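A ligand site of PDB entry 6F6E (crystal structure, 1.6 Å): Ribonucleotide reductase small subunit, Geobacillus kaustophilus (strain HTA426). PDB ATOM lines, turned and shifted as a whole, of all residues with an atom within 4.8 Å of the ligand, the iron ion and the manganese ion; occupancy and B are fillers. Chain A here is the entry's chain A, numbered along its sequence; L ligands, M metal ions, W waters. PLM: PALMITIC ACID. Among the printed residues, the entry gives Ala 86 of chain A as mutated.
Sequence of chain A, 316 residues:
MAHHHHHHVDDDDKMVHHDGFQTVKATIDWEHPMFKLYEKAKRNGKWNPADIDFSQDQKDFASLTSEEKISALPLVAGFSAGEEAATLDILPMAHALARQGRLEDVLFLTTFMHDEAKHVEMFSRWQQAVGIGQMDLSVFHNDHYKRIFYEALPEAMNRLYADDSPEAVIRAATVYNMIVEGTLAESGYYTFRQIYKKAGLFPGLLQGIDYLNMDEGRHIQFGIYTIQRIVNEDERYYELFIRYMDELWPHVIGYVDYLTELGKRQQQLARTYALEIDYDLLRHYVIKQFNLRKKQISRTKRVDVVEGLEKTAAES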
ATOM      1  N   LEU A  75     -32.267  -6.600 -17.712  1.00  0.00           N
ATOM      2  CA  LEU A  75     -30.912  -6.183 -17.426  1.00  0.00           C
ATOM      3  C   LEU A  75     -29.904  -7.095 -18.098  1.00  0.00           C
ATOM      4  O   LEU A  75     -28.918  -6.618 -18.669  1.00  0.00           O
ATOM      5  CB  LEU A  75     -30.667  -6.151 -15.918  1.00  0.00           C
ATOM      6  CG  LEU A  75     -31.327  -5.073 -15.044  1.00  0.00           C
ATOM      7  CD1 LEU A  75     -30.707  -5.124 -13.641  1.00  0.00           C
ATOM      8  CD2 LEU A  75     -31.179  -3.688 -15.626  1.00  0.00           C
ATOM      9  N   GLY A  78     -29.623  -6.318 -21.657  1.00  0.00           N
ATOM     10  CA  GLY A  78     -28.888  -5.100 -21.964  1.00  0.00           C
ATOM     11  C   GLY A  78     -27.392  -5.306 -21.885  1.00  0.00           C
ATOM     12  O   GLY A  78     -26.629  -4.737 -22.665  1.00  0.00           O
ATOM     13  N   PHE A  79     -26.949  -6.135 -20.930  1.00  0.00           N
ATOM     14  CA  PHE A  79     -25.515  -6.355 -20.773  1.00  0.00           C
ATOM     15  C   PHE A  79     -24.956  -7.297 -21.821  1.00  0.00           C
ATOM     16  O   PHE A  79     -23.878  -7.040 -22.355  1.00  0.00           O
ATOM     17  CB  PHE A  79     -25.227  -6.935 -19.410  1.00  0.00           C
ATOM     18  CG  PHE A  79     -24.831  -5.916 -18.411  1.00  0.00           C
ATOM     19  CD1 PHE A  79     -23.551  -5.383 -18.426  1.00  0.00           C
ATOM     20  CD2 PHE A  79     -25.707  -5.529 -17.400  1.00  0.00           C
ATOM     21  CE1 PHE A  79     -23.160  -4.438 -17.454  1.00  0.00           C
ATOM     22  CE2 PHE A  79     -25.330  -4.601 -16.427  1.00  0.00           C
ATOM     23  CZ  PHE A  79     -24.058  -4.052 -16.464  1.00  0.00           C
ATOM     24  N   GLY A  82     -24.647  -5.358 -24.822  1.00  0.00           N
ATOM     25  CA  GLY A  82     -23.675  -4.319 -24.573  1.00  0.00           C
ATOM     26  C   GLY A  82     -22.240  -4.808 -24.643  1.00  0.00           C
ATOM     27  O   GLY A  82     -21.367  -4.178 -25.260  1.00  0.00           O
ATOM     28  N   GLU A  83     -21.957  -5.940 -24.001  1.00  0.00           N
ATOM     29  CA  GLU A  83     -20.613  -6.495 -24.031  1.00  0.00           C
ATOM     30  C   GLU A  83     -20.245  -7.034 -25.404  1.00  0.00           C
ATOM     31  O   GLU A  83     -19.071  -7.031 -25.798  1.00  0.00           O
ATOM     32  CB  GLU A  83     -20.508  -7.631 -23.018  1.00  0.00           C
ATOM     33  CG  GLU A  83     -20.987  -7.249 -21.593  1.00  0.00           C
ATOM     34  CD  GLU A  83     -20.113  -6.220 -20.878  1.00  0.00           C
ATOM     35  OE1 GLU A  83     -19.011  -5.925 -21.382  1.00  0.00           O
ATOM     36  OE2 GLU A  83     -20.575  -5.679 -19.821  1.00  0.00           O
ATOM     37  N   ALA A  86     -19.374  -4.112 -27.384  1.00  0.00           N
ATOM     38  CA  ALA A  86     -18.090  -3.614 -26.916  1.00  0.00           C
ATOM     39  C   ALA A  86     -16.946  -4.425 -27.496  1.00  0.00           C
ATOM     40  O   ALA A  86     -15.909  -3.860 -27.899  1.00  0.00           O
ATOM     41  CB  ALA A  86     -18.047  -3.629 -25.388  1.00  0.00           C
ATOM     42  N   PHE A 112      -7.953  -4.582 -22.910  1.00  0.00           N
ATOM     43  CA  PHE A 112      -9.330  -4.087 -22.988  1.00  0.00           C
ATOM     44  C   PHE A 112     -10.208  -5.037 -23.808  1.00  0.00           C
ATOM     45  O   PHE A 112     -11.269  -5.496 -23.343  1.00  0.00           O
ATOM     46  CB  PHE A 112      -9.226  -2.683 -23.603  1.00  0.00           C
ATOM     47  CG  PHE A 112     -10.479  -1.829 -23.554  1.00  0.00           C
ATOM     48  CD1 PHE A 112     -10.435  -0.568 -22.990  1.00  0.00           C
ATOM     49  CD2 PHE A 112     -11.645  -2.243 -24.160  1.00  0.00           C
ATOM     50  CE1 PHE A 112     -11.538   0.217 -22.948  1.00  0.00           C
ATOM     51  CE2 PHE A 112     -12.760  -1.433 -24.150  1.00  0.00           C
ATOM     52  CZ  PHE A 112     -12.710  -0.187 -23.536  1.00  0.00           C
ATOM     53  N   GLU A 116     -13.346  -7.556 -22.685  1.00  0.00           N
ATOM     54  CA  GLU A 116     -14.707  -7.564 -23.175  1.00  0.00           C
ATOM     55  C   GLU A 116     -15.126  -8.955 -23.643  1.00  0.00           C
ATOM     56  O   GLU A 116     -16.283  -9.343 -23.478  1.00  0.00           O
ATOM     57  CB  GLU A 116     -14.886  -6.581 -24.335  1.00  0.00           C
ATOM     58  CG  GLU A 116     -14.508  -5.100 -24.035  1.00  0.00           C
ATOM     59  CD  GLU A 116     -15.322  -4.454 -22.895  1.00  0.00           C
ATOM     60  OE1 GLU A 116     -16.170  -5.112 -22.245  1.00  0.00           O
ATOM     61  OE2 GLU A 116     -15.125  -3.248 -22.711  1.00  0.00           O
ATOM     62  N   HIS A 119     -16.348 -10.617 -20.681  1.00  0.00           N
ATOM     63  CA  HIS A 119     -17.655 -10.155 -20.261  1.00  0.00           C
ATOM     64  C   HIS A 119     -18.781 -10.739 -21.107  1.00  0.00           C
ATOM     65  O   HIS A 119     -19.830 -11.094 -20.576  1.00  0.00           O
ATOM     66  CB  HIS A 119     -17.713  -8.642 -20.350  1.00  0.00           C
ATOM     67  CG  HIS A 119     -16.644  -7.967 -19.543  1.00  0.00           C
ATOM     68  ND1 HIS A 119     -16.406  -6.613 -19.586  1.00  0.00           N
ATOM     69  CD2 HIS A 119     -15.718  -8.485 -18.698  1.00  0.00           C
ATOM     70  CE1 HIS A 119     -15.371  -6.322 -18.830  1.00  0.00           C
ATOM     71  NE2 HIS A 119     -14.945  -7.442 -18.260  1.00  0.00           N
ATOM     72  N   PHE A 149     -26.816   1.325 -28.767  1.00  0.00           N
ATOM     73  CA  PHE A 149     -25.979   0.151 -28.953  1.00  0.00           C
ATOM     74  C   PHE A 149     -26.044  -0.446 -30.348  1.00  0.00           C
ATOM     75  O   PHE A 149     -25.050  -1.020 -30.819  1.00  0.00           O
ATOM     76  CB  PHE A 149     -26.368  -0.927 -27.942  1.00  0.00           C
ATOM     77  CG  PHE A 149     -25.926  -0.619 -26.539  1.00  0.00           C
ATOM     78  CD1 PHE A 149     -24.639  -0.895 -26.137  1.00  0.00           C
ATOM     79  CD2 PHE A 149     -26.788  -0.018 -25.630  1.00  0.00           C
ATOM     80  CE1 PHE A 149     -24.226  -0.590 -24.856  1.00  0.00           C
ATOM     81  CE2 PHE A 149     -26.388   0.292 -24.350  1.00  0.00           C
ATOM     82  CZ  PHE A 149     -25.114  -0.004 -23.958  1.00  0.00           C
ATOM     83  N   TYR A 176     -18.344   5.401 -26.126  1.00  0.00           N
ATOM     84  CA  TYR A 176     -17.962   4.068 -25.647  1.00  0.00           C
ATOM     85  C   TYR A 176     -17.626   4.101 -24.164  1.00  0.00           C
ATOM     86  O   TYR A 176     -18.207   3.358 -23.364  1.00  0.00           O
ATOM     87  CB  TYR A 176     -16.775   3.555 -26.462  1.00  0.00           C
ATOM     88  CG  TYR A 176     -16.441   2.097 -26.360  1.00  0.00           C
ATOM     89  CD1 TYR A 176     -16.432   1.302 -27.478  1.00  0.00           C
ATOM     90  CD2 TYR A 176     -16.081   1.540 -25.164  1.00  0.00           C
ATOM     91  CE1 TYR A 176     -16.116  -0.033 -27.425  1.00  0.00           C
ATOM     92  CE2 TYR A 176     -15.757   0.188 -25.089  1.00  0.00           C
ATOM     93  CZ  TYR A 176     -15.761  -0.580 -26.219  1.00  0.00           C
ATOM     94  OH  TYR A 176     -15.436  -1.932 -26.154  1.00  0.00           O
ATOM     95  N   VAL A 180     -21.460   4.529 -22.466  1.00  0.00           N
ATOM     96  CA  VAL A 180     -21.775   3.104 -22.383  1.00  0.00           C
ATOM     97  C   VAL A 180     -21.161   2.470 -21.128  1.00  0.00           C
ATOM     98  O   VAL A 180     -21.845   1.794 -20.357  1.00  0.00           O
ATOM     99  CB  VAL A 180     -21.345   2.379 -23.672  1.00  0.00           C
ATOM    100  CG1 VAL A 180     -21.338   0.850 -23.465  1.00  0.00           C
ATOM    101  CG2 VAL A 180     -22.293   2.802 -24.815  1.00  0.00           C
ATOM    102  N   GLU A 181     -19.852   2.677 -20.903  1.00  0.00           N
ATOM    103  CA  GLU A 181     -19.199   2.079 -19.727  1.00  0.00           C
ATOM    104  C   GLU A 181     -19.422   2.931 -18.484  1.00  0.00           C
ATOM    105  O   GLU A 181     -19.817   2.420 -17.425  1.00  0.00           O
ATOM    106  CB  GLU A 181     -17.698   1.926 -19.983  1.00  0.00           C
ATOM    107  CG  GLU A 181     -17.403   0.953 -21.094  1.00  0.00           C
ATOM    108  CD  GLU A 181     -15.972   0.805 -21.394  1.00  0.00           C
ATOM    109  OE1 GLU A 181     -15.172   1.769 -21.241  1.00  0.00           O
ATOM    110  OE2 GLU A 181     -15.623  -0.307 -21.822  1.00  0.00           O
ATOM    111  N   LEU A 184     -23.951   3.855 -18.218  1.00  0.00           N
ATOM    112  CA  LEU A 184     -24.858   2.723 -18.228  1.00  0.00           C
ATOM    113  C   LEU A 184     -24.277   1.515 -17.524  1.00  0.00           C
ATOM    114  O   LEU A 184     -24.912   0.932 -16.625  1.00  0.00           O
ATOM    115  CB  LEU A 184     -25.212   2.378 -19.673  1.00  0.00           C
ATOM    116  CG  LEU A 184     -26.224   3.347 -20.269  1.00  0.00           C
ATOM    117  CD1 LEU A 184     -26.307   3.049 -21.772  1.00  0.00           C
ATOM    118  CD2 LEU A 184     -27.581   3.160 -19.595  1.00  0.00           C
ATOM    119  N   ALA A 185     -23.075   1.079 -17.921  1.00  0.00           N
ATOM    120  CA  ALA A 185     -22.551  -0.145 -17.319  1.00  0.00           C
ATOM    121  C   ALA A 185     -22.411   0.002 -15.814  1.00  0.00           C
ATOM    122  O   ALA A 185     -22.799  -0.893 -15.054  1.00  0.00           O
ATOM    123  CB  ALA A 185     -21.205  -0.522 -17.912  1.00  0.00           C
ATOM    124  N   SER A 187     -23.988   1.945 -13.789  1.00  0.00           N
ATOM    125  CA  SER A 187     -25.293   1.919 -13.131  1.00  0.00           C
ATOM    126  C   SER A 187     -25.912   0.540 -13.159  1.00  0.00           C
ATOM    127  O   SER A 187     -26.638   0.172 -12.238  1.00  0.00           O
ATOM    128  CB  SER A 187     -26.228   2.936 -13.775  1.00  0.00           C
ATOM    129  OG  SER A 187     -25.632   4.206 -13.701  1.00  0.00           O
ATOM    130  N   GLY A 188     -25.607  -0.262 -14.200  1.00  0.00           N
ATOM    131  CA  GLY A 188     -26.056  -1.643 -14.228  1.00  0.00           C
ATOM    132  C   GLY A 188     -25.416  -2.530 -13.178  1.00  0.00           C
ATOM    133  O   GLY A 188     -26.082  -3.381 -12.577  1.00  0.00           O
ATOM    134  N   THR A 191     -27.193  -1.522  -9.897  1.00  0.00           N
ATOM    135  CA  THR A 191     -28.548  -2.040  -9.907  1.00  0.00           C
ATOM    136  C   THR A 191     -28.556  -3.524  -9.613  1.00  0.00           C
ATOM    137  O   THR A 191     -29.387  -4.004  -8.831  1.00  0.00           O
ATOM    138  CB  THR A 191     -29.197  -1.784 -11.263  1.00  0.00           C
ATOM    139  OG1 THR A 191     -29.204  -0.382 -11.503  1.00  0.00           O
ATOM    140  CG2 THR A 191     -30.626  -2.265 -11.319  1.00  0.00           C
ATOM    141  N   LEU A 212     -16.043  -8.127 -13.540  1.00  0.00           N
ATOM    142  CA  LEU A 212     -16.267  -7.232 -14.657  1.00  0.00           C
ATOM    143  C   LEU A 212     -16.170  -5.762 -14.222  1.00  0.00           C
ATOM    144  O   LEU A 212     -15.557  -4.936 -14.916  1.00  0.00           O
ATOM    145  CB  LEU A 212     -17.643  -7.571 -15.229  1.00  0.00           C
ATOM    146  CG  LEU A 212     -18.248  -6.831 -16.350  1.00  0.00           C
ATOM    147  CD1 LEU A 212     -19.349  -7.713 -16.996  1.00  0.00           C
ATOM    148  CD2 LEU A 212     -18.836  -5.595 -15.782  1.00  0.00           C
ATOM    149  N   GLU A 216     -13.629  -2.885 -15.701  1.00  0.00           N
ATOM    150  CA  GLU A 216     -14.162  -1.706 -16.371  1.00  0.00           C
ATOM    151  C   GLU A 216     -13.587  -0.424 -15.768  1.00  0.00           C
ATOM    152  O   GLU A 216     -13.506   0.577 -16.462  1.00  0.00           O
ATOM    153  CB  GLU A 216     -15.687  -1.709 -16.349  1.00  0.00           C
ATOM    154  CG  GLU A 216     -16.256  -2.856 -17.251  1.00  0.00           C
ATOM    155  CD  GLU A 216     -15.972  -2.629 -18.702  1.00  0.00           C
ATOM    156  OE1 GLU A 216     -15.909  -1.440 -19.076  1.00  0.00           O
ATOM    157  OE2 GLU A 216     -15.804  -3.616 -19.479  1.00  0.00           O
ATOM    158  N   HIS A 219     -11.014   0.460 -18.096  1.00  0.00           N
ATOM    159  CA  HIS A 219     -11.554   0.892 -19.385  1.00  0.00           C
ATOM    160  C   HIS A 219     -11.970   2.367 -19.312  1.00  0.00           C
ATOM    161  O   HIS A 219     -11.706   3.161 -20.235  1.00  0.00           O
ATOM    162  CB  HIS A 219     -12.750   0.050 -19.779  1.00  0.00           C
ATOM    163  CG  HIS A 219     -12.433  -1.383 -19.940  1.00  0.00           C
ATOM    164  ND1 HIS A 219     -13.259  -2.269 -20.601  1.00  0.00           N
ATOM    165  CD2 HIS A 219     -11.347  -2.093 -19.546  1.00  0.00           C
ATOM    166  CE1 HIS A 219     -12.713  -3.483 -20.540  1.00  0.00           C
ATOM    167  NE2 HIS A 219     -11.544  -3.396 -19.935  1.00  0.00           N
ATOM    168  N   TYR A 255     -33.716   4.808 -21.901  1.00  0.00           N
ATOM    169  CA  TYR A 255     -33.592   3.378 -21.653  1.00  0.00           C
ATOM    170  C   TYR A 255     -33.765   3.089 -20.162  1.00  0.00           C
ATOM    171  O   TYR A 255     -34.461   2.134 -19.797  1.00  0.00           O
ATOM    172  CB  TYR A 255     -32.248   2.870 -22.178  1.00  0.00           C
ATOM    173  CG  TYR A 255     -31.919   1.431 -21.827  1.00  0.00           C
ATOM    174  CD1 TYR A 255     -32.719   0.396 -22.277  1.00  0.00           C
ATOM    175  CD2 TYR A 255     -30.814   1.114 -21.052  1.00  0.00           C
ATOM    176  CE1 TYR A 255     -32.436  -0.911 -21.956  1.00  0.00           C
ATOM    177  CE2 TYR A 255     -30.510  -0.214 -20.719  1.00  0.00           C
ATOM    178  CZ  TYR A 255     -31.336  -1.219 -21.182  1.00  0.00           C
ATOM    179  OH  TYR A 255     -31.065  -2.545 -20.880  1.00  0.00           O
ATOM    180  N   VAL A 256     -33.210   3.941 -19.295  1.00  0.00           N
ATOM    181  CA  VAL A 256     -33.391   3.756 -17.860  1.00  0.00           C
ATOM    182  C   VAL A 256     -34.876   3.850 -17.480  1.00  0.00           C
ATOM    183  O   VAL A 256     -35.352   3.097 -16.633  1.00  0.00           O
ATOM    184  CB  VAL A 256     -32.543   4.788 -17.086  1.00  0.00           C
ATOM    185  CG1 VAL A 256     -32.934   4.848 -15.608  1.00  0.00           C
ATOM    186  CG2 VAL A 256     -31.050   4.427 -17.210  1.00  0.00           C
ATOM    187  N   LEU A 259     -36.524   0.442 -18.498  1.00  0.00           N
ATOM    188  CA  LEU A 259     -36.239  -0.626 -17.528  1.00  0.00           C
ATOM    189  C   LEU A 259     -36.959  -0.380 -16.219  1.00  0.00           C
ATOM    190  O   LEU A 259     -37.420  -1.323 -15.571  1.00  0.00           O
ATOM    191  CB  LEU A 259     -34.746  -0.727 -17.265  1.00  0.00           C
ATOM    192  CG  LEU A 259     -33.916  -1.276 -18.419  1.00  0.00           C
ATOM    193  CD1 LEU A 259     -32.473  -1.185 -17.979  1.00  0.00           C
ATOM    194  CD2 LEU A 259     -34.315  -2.714 -18.753  1.00  0.00           C
ATOM    195  N   THR A 260     -37.015   0.885 -15.792  1.00  0.00           N
ATOM    196  CA  THR A 260     -37.729   1.251 -14.570  1.00  0.00           C
ATOM    197  C   THR A 260     -39.202   0.900 -14.687  1.00  0.00           C
ATOM    198  O   THR A 260     -39.793   0.319 -13.775  1.00  0.00           O
ATOM    199  CB  THR A 260     -37.560   2.743 -14.314  1.00  0.00           C
ATOM    200  OG1 THR A 260     -36.277   2.958 -13.709  1.00  0.00           O
ATOM    201  CG2 THR A 260     -38.640   3.286 -13.414  1.00  0.00           C
ATOM    202  N   TYR A 279     -36.375   2.418  -7.474  1.00  0.00           N
ATOM    203  CA  TYR A 279     -35.976   2.828  -8.808  1.00  0.00           C
ATOM    204  C   TYR A 279     -35.667   4.308  -8.884  1.00  0.00           C
ATOM    205  O   TYR A 279     -34.909   4.719  -9.756  1.00  0.00           O
ATOM    206  CB  TYR A 279     -37.057   2.490  -9.836  1.00  0.00           C
ATOM    207  CG  TYR A 279     -37.247   1.009  -9.964  1.00  0.00           C
ATOM    208  CD1 TYR A 279     -36.336   0.238 -10.650  1.00  0.00           C
ATOM    209  CD2 TYR A 279     -38.325   0.384  -9.369  1.00  0.00           C
ATOM    210  CE1 TYR A 279     -36.490  -1.119 -10.753  1.00  0.00           C
ATOM    211  CE2 TYR A 279     -38.502  -0.973  -9.463  1.00  0.00           C
ATOM    212  CZ  TYR A 279     -37.581  -1.719 -10.170  1.00  0.00           C
ATOM    213  OH  TYR A 279     -37.745  -3.080 -10.254  1.00  0.00           O
ATOM    214  N   LEU A 282     -32.109   4.396  -8.060  1.00  0.00           N
ATOM    215  CA  LEU A 282     -31.353   3.922  -9.213  1.00  0.00           C
ATOM    216  C   LEU A 282     -31.270   5.005 -10.282  1.00  0.00           C
ATOM    217  O   LEU A 282     -30.185   5.375 -10.732  1.00  0.00           O
ATOM    218  CB  LEU A 282     -31.983   2.659  -9.790  1.00  0.00           C
ATOM    219  CG  LEU A 282     -31.980   1.464  -8.840  1.00  0.00           C
ATOM    220  CD1 LEU A 282     -32.795   0.316  -9.454  1.00  0.00           C
ATOM    221  CD2 LEU A 282     -30.558   1.017  -8.481  1.00  0.00           C
ATOM    222  N   VAL A 286     -27.875   6.829 -11.943  1.00  0.00           N
ATOM    223  CA  VAL A 286     -27.541   7.086 -13.343  1.00  0.00           C
ATOM    224  C   VAL A 286     -27.202   8.559 -13.547  1.00  0.00           C
ATOM    225  O   VAL A 286     -26.201   8.903 -14.190  1.00  0.00           O
ATOM    226  CB  VAL A 286     -28.675   6.650 -14.267  1.00  0.00           C
ATOM    227  CG1 VAL A 286     -28.302   6.900 -15.724  1.00  0.00           C
ATOM    228  CG2 VAL A 286     -28.995   5.185 -14.083  1.00  0.00           C
HETATM  229  C1  PLM L   1     -18.318  -2.190 -22.184  1.00  0.00           C
HETATM  230  O1  PLM L   1     -17.578  -2.700 -21.310  1.00  0.00           O
HETATM  231  O2  PLM L   1     -18.053  -1.235 -22.955  1.00  0.00           O
HETATM  232  C2  PLM L   1     -19.802  -2.734 -22.370  1.00  0.00           C
HETATM  233  C3  PLM L   1     -20.813  -2.310 -21.300  1.00  0.00           C
HETATM  234  C4  PLM L   1     -22.241  -2.669 -21.653  1.00  0.00           C
HETATM  235  C5  PLM L   1     -23.303  -2.258 -20.555  1.00  0.00           C
HETATM  236  C6  PLM L   1     -24.717  -2.096 -21.118  1.00  0.00           C
HETATM  237  C7  PLM L   1     -25.960  -2.655 -20.326  1.00  0.00           C
HETATM  238  C8  PLM L   1     -26.125  -2.157 -18.939  1.00  0.00           C
HETATM  239  C9  PLM L   1     -27.618  -2.055 -18.420  1.00  0.00           C
HETATM  240  CA  PLM L   1     -27.774  -0.746 -17.660  1.00  0.00           C
HETATM  241  CB  PLM L   1     -28.897  -0.623 -16.639  1.00  0.00           C
HETATM  242  CC  PLM L   1     -29.052   0.851 -16.199  1.00  0.00           C
HETATM  243  CD  PLM L   1     -29.679   1.087 -14.794  1.00  0.00           C
HETATM  244  CE  PLM L   1     -31.209   1.010 -14.799  1.00  0.00           C
HETATM  245  CF  PLM L   1     -31.881   1.463 -13.489  1.00  0.00           C
HETATM  246  CG  PLM L   1     -33.324   1.021 -13.398  1.00  0.00           C
HETATM  247 FE    FE M   1     -15.363  -2.088 -21.095  1.00  0.00          FE
HETATM  248 MN    MN M   2     -17.339  -4.895 -20.520  1.00  0.00          MN
HETATM  249  O   HOH W   1     -18.701  -4.265 -18.879  1.00  0.00           O
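The iron ion is bound by the side-chain carboxylate (OE2) of Glu 181 (1.9 Å), the side-chain carboxylate (OE2) of Glu 116 (2.0 Å), a ring nitrogen (ND1) of His 219 (2.2 Å), the side-chain carboxylate (OE1) of Glu 216 (2.2 Å), the side-chain carboxylate (OE2) of Glu 216 (2.3 Å) and an oxygen (O1) of the ligand (2.3 Å).
Within 4 Å of the manganese ion: Glu 83, Glu 116, His 119 and Glu 216. The nearest printed residue that does not touch the manganese ion is Leu 212 (4.7 Å).
The manganese ion is bound by OE1 of Glu 116 (2.1 Å), OE1 of Glu 83 (2.1 Å), ND1 of His 119 (2.2 Å), water W1 (2.2 Å), OE2 of Glu 216 (2.3 Å) and O1 of the ligand (2.3 Å).
Leu 75 touches the ligand. Gly 78 touches the ligand (O to C7, 3.2 Å). CE2 of Phe 79 touches C8 of the ligand, 3.6 Å away. Gly 82 touches the ligand (O to C2, 3.6 Å). CB of Ala 86 touches O2 of the ligand, 3.4 Å away. Phe 149 touches the ligand (CZ to C6, 3.5 Å). Tyr 176 touches the ligand. Val 180 touches the ligand (CG1 to C3, 3.9 Å). Leu 184 touches the ligand (O to CA, 3.5 Å). Ala 185 touches the ligand (CB to C5, 3.8 Å). Gly 188 touches the ligand. Thr 191 touches the ligand. Leu 259 touches the ligand (CD1 to CB, 3.9 Å). Thr 260 touches the ligand (OG1 to CG, 3.5 Å). CB of Leu 282 touches CF of the ligand (3.9 Å). Hydrophobic or aromatic side chains that line the ligand: Leu 75, Phe 79, Ala 86, Phe 149, Tyr 176, Val 180, Ala 185, Leu 259 and Leu 282. The nearest printed residue that does not touch the ligand is Ser 187 (4.05 Å).
The backbone NH of Glu 181 is in hydrogen-bond range of the backbone carbonyl oxygen of Tyr 176, 3.0 Å away. O of Ala 86 lies within hydrogen-bond range of OH of Tyr 176, at 2.6 Å. OG1 of Thr 260 sits at hydrogen-bond distance from O of Val 256, 3.1 Å away. O of Ser 187 lies within hydrogen-bond range of OG1 of Thr 191. The backbone carbonyl oxygen (O) of Val 180 lies within hydrogen-bond range of the backbone NH (N) of Ala 185, 2.8 Å away.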
